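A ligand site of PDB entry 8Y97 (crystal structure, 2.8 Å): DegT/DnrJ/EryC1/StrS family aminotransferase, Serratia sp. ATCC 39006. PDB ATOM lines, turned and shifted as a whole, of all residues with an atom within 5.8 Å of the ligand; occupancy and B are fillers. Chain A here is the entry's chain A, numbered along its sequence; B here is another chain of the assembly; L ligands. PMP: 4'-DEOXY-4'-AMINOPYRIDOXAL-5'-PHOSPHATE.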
ATOM      1  N   SER A  84     -19.045 -23.482  29.897  1.00  0.00           N
ATOM      2  CA  SER A  84     -17.623 -23.197  29.794  1.00  0.00           C
ATOM      3  C   SER A  84     -16.926 -24.232  28.926  1.00  0.00           C
ATOM      4  O   SER A  84     -17.456 -25.318  28.691  1.00  0.00           O
ATOM      5  CB  SER A  84     -16.993 -23.148  31.158  1.00  0.00           C
ATOM      6  OG  SER A  84     -17.083 -24.421  31.789  1.00  0.00           O
ATOM      7  N   GLY A  85     -15.715 -23.878  28.467  1.00  0.00           N
ATOM      8  CA  GLY A  85     -14.850 -24.810  27.773  1.00  0.00           C
ATOM      9  C   GLY A  85     -14.364 -25.934  28.701  1.00  0.00           C
ATOM     10  O   GLY A  85     -14.232 -27.074  28.271  1.00  0.00           O
ATOM     11  N   THR A  86     -14.104 -25.589  29.967  1.00  0.00           N
ATOM     12  CA  THR A  86     -13.613 -26.549  30.943  1.00  0.00           C
ATOM     13  C   THR A  86     -14.642 -27.669  31.104  1.00  0.00           C
ATOM     14  O   THR A  86     -14.288 -28.845  31.139  1.00  0.00           O
ATOM     15  CB  THR A  86     -13.339 -25.862  32.272  1.00  0.00           C
ATOM     16  OG1 THR A  86     -12.537 -24.719  31.967  1.00  0.00           O
ATOM     17  CG2 THR A  86     -12.600 -26.751  33.250  1.00  0.00           C
ATOM     18  N   SER A  87     -15.917 -27.281  31.198  1.00  0.00           N
ATOM     19  CA  SER A  87     -17.015 -28.226  31.380  1.00  0.00           C
ATOM     20  C   SER A  87     -17.200 -29.085  30.131  1.00  0.00           C
ATOM     21  O   SER A  87     -17.531 -30.268  30.246  1.00  0.00           O
ATOM     22  CB  SER A  87     -18.276 -27.518  31.762  1.00  0.00           C
ATOM     23  OG  SER A  87     -18.479 -26.364  30.959  1.00  0.00           O
ATOM     24  N   LEU A  89     -14.865 -30.035  28.010  1.00  0.00           N
ATOM     25  CA  LEU A  89     -13.786 -31.007  27.995  1.00  0.00           C
ATOM     26  C   LEU A  89     -14.070 -32.123  28.997  1.00  0.00           C
ATOM     27  O   LEU A  89     -13.823 -33.292  28.711  1.00  0.00           O
ATOM     28  CB  LEU A  89     -12.453 -30.302  28.299  1.00  0.00           C
ATOM     29  CG  LEU A  89     -11.975 -29.288  27.263  1.00  0.00           C
ATOM     30  CD1 LEU A  89     -10.881 -28.403  27.839  1.00  0.00           C
ATOM     31  CD2 LEU A  89     -11.486 -29.968  25.995  1.00  0.00           C
ATOM     32  N   THR A 110      -0.208 -26.171  27.985  1.00  0.00           N
ATOM     33  CA  THR A 110      -1.554 -25.762  27.595  1.00  0.00           C
ATOM     34  C   THR A 110      -2.130 -24.955  28.761  1.00  0.00           C
ATOM     35  O   THR A 110      -1.434 -24.728  29.745  1.00  0.00           O
ATOM     36  CB  THR A 110      -2.415 -26.981  27.240  1.00  0.00           C
ATOM     37  OG1 THR A 110      -3.724 -26.490  26.990  1.00  0.00           O
ATOM     38  CG2 THR A 110      -2.466 -28.018  28.343  1.00  0.00           C
ATOM     39  N   PHE A 111      -3.380 -24.530  28.633  1.00  0.00           N
ATOM     40  CA  PHE A 111      -4.051 -23.829  29.717  1.00  0.00           C
ATOM     41  C   PHE A 111      -4.438 -24.829  30.795  1.00  0.00           C
ATOM     42  O   PHE A 111      -4.742 -25.984  30.485  1.00  0.00           O
ATOM     43  CB  PHE A 111      -5.258 -23.041  29.186  1.00  0.00           C
ATOM     44  CG  PHE A 111      -5.858 -22.068  30.181  1.00  0.00           C
ATOM     45  CD1 PHE A 111      -5.162 -20.921  30.561  1.00  0.00           C
ATOM     46  CD2 PHE A 111      -7.123 -22.274  30.727  1.00  0.00           C
ATOM     47  CE1 PHE A 111      -5.714 -20.020  31.470  1.00  0.00           C
ATOM     48  CE2 PHE A 111      -7.676 -21.374  31.612  1.00  0.00           C
ATOM     49  CZ  PHE A 111      -6.969 -20.249  31.987  1.00  0.00           C
ATOM     50  N   ALA A 113      -6.976 -25.390  32.395  1.00  0.00           N
ATOM     51  CA  ALA A 113      -8.319 -25.948  32.276  1.00  0.00           C
ATOM     52  C   ALA A 113      -8.323 -27.285  31.534  1.00  0.00           C
ATOM     53  O   ALA A 113      -9.218 -28.099  31.747  1.00  0.00           O
ATOM     54  CB  ALA A 113      -9.232 -24.952  31.597  1.00  0.00           C
ATOM     55  N   THR A 114      -7.354 -27.493  30.631  1.00  0.00           N
ATOM     56  CA  THR A 114      -7.253 -28.753  29.902  1.00  0.00           C
ATOM     57  C   THR A 114      -7.102 -29.890  30.905  1.00  0.00           C
ATOM     58  O   THR A 114      -7.868 -30.847  30.878  1.00  0.00           O
ATOM     59  CB  THR A 114      -6.062 -28.721  28.932  1.00  0.00           C
ATOM     60  OG1 THR A 114      -6.079 -27.477  28.249  1.00  0.00           O
ATOM     61  CG2 THR A 114      -6.106 -29.867  27.929  1.00  0.00           C
ATOM     62  N   VAL A 156      -4.005 -30.772  22.196  1.00  0.00           N
ATOM     63  CA  VAL A 156      -4.510 -29.405  22.200  1.00  0.00           C
ATOM     64  C   VAL A 156      -4.116 -28.738  20.889  1.00  0.00           C
ATOM     65  O   VAL A 156      -2.929 -28.723  20.535  1.00  0.00           O
ATOM     66  CB  VAL A 156      -3.996 -28.596  23.398  1.00  0.00           C
ATOM     67  CG1 VAL A 156      -4.556 -27.170  23.411  1.00  0.00           C
ATOM     68  CG2 VAL A 156      -4.296 -29.285  24.731  1.00  0.00           C
ATOM     69  N   VAL A 158      -3.275 -25.882  20.036  1.00  0.00           N
ATOM     70  CA  VAL A 158      -2.891 -24.691  20.790  1.00  0.00           C
ATOM     71  C   VAL A 158      -2.550 -23.569  19.807  1.00  0.00           C
ATOM     72  O   VAL A 158      -1.953 -23.821  18.763  1.00  0.00           O
ATOM     73  CB  VAL A 158      -1.717 -24.990  21.753  1.00  0.00           C
ATOM     74  CG1 VAL A 158      -0.400 -25.219  21.025  1.00  0.00           C
ATOM     75  CG2 VAL A 158      -1.558 -23.887  22.795  1.00  0.00           C
ATOM     76  N   ASP A 182      -8.896 -30.744  22.378  1.00  0.00           N
ATOM     77  CA  ASP A 182      -9.151 -29.444  22.977  1.00  0.00           C
ATOM     78  C   ASP A 182      -9.058 -28.390  21.870  1.00  0.00           C
ATOM     79  O   ASP A 182      -7.958 -27.993  21.483  1.00  0.00           O
ATOM     80  CB  ASP A 182      -8.205 -29.157  24.132  1.00  0.00           C
ATOM     81  CG  ASP A 182      -8.529 -27.921  24.954  1.00  0.00           C
ATOM     82  OD1 ASP A 182      -9.441 -27.164  24.561  1.00  0.00           O
ATOM     83  OD2 ASP A 182      -7.862 -27.708  25.987  1.00  0.00           O
ATOM     84  N   SER A 184     -10.230 -25.300  21.913  1.00  0.00           N
ATOM     85  CA  SER A 184     -10.628 -24.043  22.538  1.00  0.00           C
ATOM     86  C   SER A 184      -9.943 -22.860  21.858  1.00  0.00           C
ATOM     87  O   SER A 184     -10.335 -21.710  22.107  1.00  0.00           O
ATOM     88  CB  SER A 184     -10.333 -24.063  24.013  1.00  0.00           C
ATOM     89  OG  SER A 184     -11.252 -24.902  24.700  1.00  0.00           O
ATOM     90  N   HIS A 185      -8.930 -23.115  21.032  1.00  0.00           N
ATOM     91  CA  HIS A 185      -8.295 -22.067  20.244  1.00  0.00           C
ATOM     92  C   HIS A 185      -8.585 -22.227  18.758  1.00  0.00           C
ATOM     93  O   HIS A 185      -8.391 -21.283  17.989  1.00  0.00           O
ATOM     94  CB  HIS A 185      -6.788 -22.068  20.494  1.00  0.00           C
ATOM     95  CG  HIS A 185      -6.407 -21.689  21.881  1.00  0.00           C
ATOM     96  ND1 HIS A 185      -5.179 -22.007  22.419  1.00  0.00           N
ATOM     97  CD2 HIS A 185      -7.054 -21.001  22.821  1.00  0.00           C
ATOM     98  CE1 HIS A 185      -5.098 -21.513  23.645  1.00  0.00           C
ATOM     99  NE2 HIS A 185      -6.235 -20.908  23.910  1.00  0.00           N
ATOM    100  N   SER A 206     -13.931 -24.124  24.191  1.00  0.00           N
ATOM    101  CA  SER A 206     -14.311 -22.867  24.806  1.00  0.00           C
ATOM    102  C   SER A 206     -15.001 -21.985  23.772  1.00  0.00           C
ATOM    103  O   SER A 206     -14.573 -21.924  22.621  1.00  0.00           O
ATOM    104  CB  SER A 206     -13.109 -22.174  25.392  1.00  0.00           C
ATOM    105  OG  SER A 206     -13.443 -20.885  25.908  1.00  0.00           O
ATOM    106  N   LEU A 207     -16.079 -21.318  24.192  1.00  0.00           N
ATOM    107  CA  LEU A 207     -16.758 -20.327  23.376  1.00  0.00           C
ATOM    108  C   LEU A 207     -16.773 -19.008  24.145  1.00  0.00           C
ATOM    109  O   LEU A 207     -17.743 -18.250  24.085  1.00  0.00           O
ATOM    110  CB  LEU A 207     -18.169 -20.792  23.040  1.00  0.00           C
ATOM    111  CG  LEU A 207     -18.262 -22.019  22.127  1.00  0.00           C
ATOM    112  CD1 LEU A 207     -19.695 -22.529  22.058  1.00  0.00           C
ATOM    113  CD2 LEU A 207     -17.756 -21.693  20.731  1.00  0.00           C
ATOM    114  N   MET A 208     -15.675 -18.740  24.867  1.00  0.00           N
ATOM    115  CA  MET A 208     -15.575 -17.561  25.705  1.00  0.00           C
ATOM    116  C   MET A 208     -15.360 -16.338  24.817  1.00  0.00           C
ATOM    117  O   MET A 208     -15.004 -16.482  23.637  1.00  0.00           O
ATOM    118  CB  MET A 208     -14.430 -17.712  26.716  1.00  0.00           C
ATOM    119  CG  MET A 208     -14.607 -16.866  27.968  1.00  0.00           C
ATOM    120  SD  MET A 208     -13.102 -16.016  28.478  1.00  0.00           S
ATOM    121  CE  MET A 208     -13.833 -14.579  29.266  1.00  0.00           C
ATOM    122  N   ASP A 210     -13.125 -14.291  24.565  1.00  0.00           N
ATOM    123  CA  ASP A 210     -11.747 -14.018  24.171  1.00  0.00           C
ATOM    124  C   ASP A 210     -11.304 -14.996  23.077  1.00  0.00           C
ATOM    125  O   ASP A 210     -10.116 -15.094  22.795  1.00  0.00           O
ATOM    126  CB  ASP A 210     -10.808 -14.035  25.363  1.00  0.00           C
ATOM    127  CG  ASP A 210     -10.566 -15.381  26.030  1.00  0.00           C
ATOM    128  OD1 ASP A 210     -11.237 -16.360  25.652  1.00  0.00           O
ATOM    129  OD2 ASP A 210      -9.672 -15.444  26.904  1.00  0.00           O
ATOM    130  N   LYS A 211     -12.261 -15.691  22.460  1.00  0.00           N
ATOM    131  CA  LYS A 211     -11.970 -16.649  21.402  1.00  0.00           C
ATOM    132  C   LYS A 211     -12.433 -16.103  20.056  1.00  0.00           C
ATOM    133  O   LYS A 211     -13.326 -15.271  19.998  1.00  0.00           O
ATOM    134  CB  LYS A 211     -12.652 -17.998  21.692  1.00  0.00           C
ATOM    135  CG  LYS A 211     -12.289 -18.639  23.014  1.00  0.00           C
ATOM    136  CD  LYS A 211     -10.790 -18.625  23.313  1.00  0.00           C
ATOM    137  CE  LYS A 211     -10.347 -19.506  24.440  1.00  0.00           C
ATOM    138  NZ  LYS A 211     -11.209 -19.441  25.626  1.00  0.00           N
ATOM    139  N   GLU A 218     -19.071 -16.199  29.233  1.00  0.00           N
ATOM    140  CA  GLU A 218     -18.572 -17.552  29.450  1.00  0.00           C
ATOM    141  C   GLU A 218     -19.497 -18.528  28.734  1.00  0.00           C
ATOM    142  O   GLU A 218     -20.721 -18.388  28.808  1.00  0.00           O
ATOM    143  CB  GLU A 218     -18.507 -17.851  30.953  1.00  0.00           C
ATOM    144  CG  GLU A 218     -17.616 -16.894  31.729  1.00  0.00           C
ATOM    145  CD  GLU A 218     -16.123 -17.043  31.520  1.00  0.00           C
ATOM    146  OE1 GLU A 218     -15.704 -18.071  30.939  1.00  0.00           O
ATOM    147  OE2 GLU A 218     -15.389 -16.133  31.942  1.00  0.00           O
ATOM    148  N   ALA A 219     -18.903 -19.513  28.060  1.00  0.00           N
ATOM    149  CA  ALA A 219     -19.644 -20.536  27.342  1.00  0.00           C
ATOM    150  C   ALA A 219     -18.683 -21.545  26.731  1.00  0.00           C
ATOM    151  O   ALA A 219     -17.486 -21.285  26.610  1.00  0.00           O
ATOM    152  CB  ALA A 219     -20.511 -19.905  26.268  1.00  0.00           C
ATOM    153  N   GLY A 220     -19.220 -22.707  26.328  1.00  0.00           N
ATOM    154  CA  GLY A 220     -18.454 -23.727  25.650  1.00  0.00           C
ATOM    155  C   GLY A 220     -19.376 -24.741  24.978  1.00  0.00           C
ATOM    156  O   GLY A 220     -20.590 -24.648  25.086  1.00  0.00           O
ATOM    157  N   TRP A 338       1.998 -16.376  27.012  1.00  0.00           N
ATOM    158  CA  TRP A 338       0.698 -16.966  27.301  1.00  0.00           C
ATOM    159  C   TRP A 338       0.775 -17.786  28.580  1.00  0.00           C
ATOM    160  O   TRP A 338       0.037 -17.533  29.533  1.00  0.00           O
ATOM    161  CB  TRP A 338       0.201 -17.830  26.129  1.00  0.00           C
ATOM    162  CG  TRP A 338      -1.152 -18.421  26.386  1.00  0.00           C
ATOM    163  CD1 TRP A 338      -2.250 -17.759  26.853  1.00  0.00           C
ATOM    164  CD2 TRP A 338      -1.547 -19.797  26.238  1.00  0.00           C
ATOM    165  NE1 TRP A 338      -3.304 -18.621  26.999  1.00  0.00           N
ATOM    166  CE2 TRP A 338      -2.902 -19.879  26.632  1.00  0.00           C
ATOM    167  CE3 TRP A 338      -0.899 -20.960  25.810  1.00  0.00           C
ATOM    168  CZ2 TRP A 338      -3.610 -21.070  26.600  1.00  0.00           C
ATOM    169  CZ3 TRP A 338      -1.610 -22.146  25.795  1.00  0.00           C
ATOM    170  CH2 TRP A 338      -2.943 -22.199  26.190  1.00  0.00           C
ATOM    171  N   PHE B 165      -9.043 -18.439  37.204  1.00  0.00           N
ATOM    172  CA  PHE B 165      -9.079 -16.979  37.180  1.00  0.00           C
ATOM    173  C   PHE B 165     -10.153 -16.488  38.150  1.00  0.00           C
ATOM    174  O   PHE B 165     -11.213 -16.043  37.724  1.00  0.00           O
ATOM    175  CB  PHE B 165      -9.311 -16.402  35.778  1.00  0.00           C
ATOM    176  CG  PHE B 165      -8.166 -16.542  34.767  1.00  0.00           C
ATOM    177  CD1 PHE B 165      -6.831 -16.440  35.152  1.00  0.00           C
ATOM    178  CD2 PHE B 165      -8.448 -16.802  33.429  1.00  0.00           C
ATOM    179  CE1 PHE B 165      -5.814 -16.569  34.221  1.00  0.00           C
ATOM    180  CE2 PHE B 165      -7.426 -16.926  32.509  1.00  0.00           C
ATOM    181  CZ  PHE B 165      -6.112 -16.812  32.899  1.00  0.00           C
ATOM    182  N   ASN B 190     -14.414 -23.797  35.776  1.00  0.00           N
ATOM    183  CA  ASN B 190     -14.800 -22.481  35.303  1.00  0.00           C
ATOM    184  C   ASN B 190     -16.238 -22.218  35.730  1.00  0.00           C
ATOM    185  O   ASN B 190     -17.181 -22.610  35.048  1.00  0.00           O
ATOM    186  CB  ASN B 190     -14.633 -22.311  33.793  1.00  0.00           C
ATOM    187  CG  ASN B 190     -14.953 -20.907  33.346  1.00  0.00           C
ATOM    188  OD1 ASN B 190     -15.266 -20.039  34.165  1.00  0.00           O
ATOM    189  ND2 ASN B 190     -14.867 -20.644  32.051  1.00  0.00           N
ATOM    190  N   ARG B 192     -16.911 -18.980  36.474  1.00  0.00           N
ATOM    191  CA  ARG B 192     -16.951 -17.537  36.271  1.00  0.00           C
ATOM    192  C   ARG B 192     -18.278 -17.175  35.598  1.00  0.00           C
ATOM    193  O   ARG B 192     -18.728 -17.897  34.715  1.00  0.00           O
ATOM    194  CB  ARG B 192     -15.800 -17.055  35.383  1.00  0.00           C
ATOM    195  CG  ARG B 192     -14.394 -17.360  35.874  1.00  0.00           C
ATOM    196  CD  ARG B 192     -13.331 -16.580  35.088  1.00  0.00           C
ATOM    197  NE  ARG B 192     -13.359 -16.882  33.647  1.00  0.00           N
ATOM    198  CZ  ARG B 192     -12.871 -17.971  33.060  1.00  0.00           C
ATOM    199  NH1 ARG B 192     -12.209 -18.880  33.749  1.00  0.00           N
ATOM    200  NH2 ARG B 192     -13.025 -18.125  31.759  1.00  0.00           N
HETATM  201  N1  PMP L   1      -8.500 -24.402  26.990  1.00  0.00           N
HETATM  202  C2  PMP L   1      -7.658 -23.474  26.525  1.00  0.00           C
HETATM  203  C2A PMP L   1      -6.638 -23.894  25.506  1.00  0.00           C
HETATM  204  C3  PMP L   1      -7.726 -22.151  26.990  1.00  0.00           C
HETATM  205  O3  PMP L   1      -6.854 -21.193  26.522  1.00  0.00           O
HETATM  206  C4  PMP L   1      -8.690 -21.787  27.939  1.00  0.00           C
HETATM  207  C4A PMP L   1      -8.742 -20.370  28.463  1.00  0.00           C
HETATM  208  N4A PMP L   1      -9.965 -19.603  28.192  1.00  0.00           N
HETATM  209  C5  PMP L   1      -9.547 -22.787  28.429  1.00  0.00           C
HETATM  210  C6  PMP L   1      -9.416 -24.062  27.899  1.00  0.00           C
HETATM  211  C5A PMP L   1     -10.613 -22.506  29.434  1.00  0.00           C
HETATM  212  O4P PMP L   1     -11.910 -22.460  28.760  1.00  0.00           O
HETATM  213  P   PMP L   1     -13.174 -21.770  29.447  1.00  0.00           P
HETATM  214  O1P PMP L   1     -13.688 -22.795  30.438  1.00  0.00           O
HETATM  215  O2P PMP L   1     -14.165 -21.475  28.339  1.00  0.00           O
HETATM  216  O3P PMP L   1     -12.635 -20.516  30.116  1.00  0.00           O
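OG of Ser 206 lies within hydrogen-bond range of O2P of the ligand (2.6 Å).
An oxygen (O3) of the ligand lies within hydrogen-bond range of a ring nitrogen (NE2) of His 185 (2.7 Å).
The backbone NH (N) of Thr 86 is in hydrogen-bond range of an oxygen (O1P) of the ligand (2.9 Å).
O1P of the ligand lies within hydrogen-bond range of OG1 of Thr 86 (2.7 Å).
A nitrogen (N4A) of the ligand sits close to the side-chain amino group (NZ) of Lys 211 (2.9 Å).
N of Gly 85 is in hydrogen-bond range of O2P of the ligand (2.9 Å).
The guanidinium group (NH2) of Arg 192 of chain B lies within salt-bridge range of an oxygen (O3P) of the ligand (2.9 Å).
ND2 of Asn 190 of chain B sits at hydrogen-bond distance from O1P of the ligand, 2.9 Å away.
The side-chain hydroxyl (OG) of Ser 206 lies within hydrogen-bond range of the side-chain amino group (NZ) of Lys 211 (2.7 Å).
The side-chain hydroxyl of Ser 184 lies within hydrogen-bond range of the backbone NH of Ser 206 (2.8 Å).
OD1 of Asp 210 lies within salt-bridge range of NZ of Lys 211 (3.1 Å).
The side-chain amide nitrogen of Asn 190 of chain B is in hydrogen-bond range of the side-chain carboxylate of Glu 218, at 2.9 Å.
The backbone carbonyl oxygen (O) of Phe 111 lies within hydrogen-bond range of the side-chain hydroxyl (OG1) of Thr 114 (3.0 Å).
OD1 of Asp 182 is in hydrogen-bond range of OG of Ser 184, at 2.9 Å.
The side-chain carboxylate (OD2) of Asp 182 is in hydrogen-bond range of the side-chain hydroxyl (OG1) of Thr 114 (2.9 Å).
The backbone carbonyl oxygen of Ala 219 sits at hydrogen-bond distance from the backbone NH of Leu 207.
CB of Ser 84 touches O1P of the ligand, 3.4 Å away.
CD2 of Phe 111 touches C4 of the ligand (3.2 Å).
Ala 113 touches the ligand.
Asp 182 touches the ligand.
Ser 184 touches the ligand (CB to N1, 3.5 Å).
Ala 219 touches the ligand.
Trp 338 touches the ligand.
Hydrophobic or aromatic side chains within 4 Å of the ligand: Phe 111, Ala 113, His 185 and Trp 338.
Of the 26 residues printed, 14 come within 4 Å of the ligand.
The nearest printed residue that does not touch the ligand is Glu 218 (4.01 Å).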
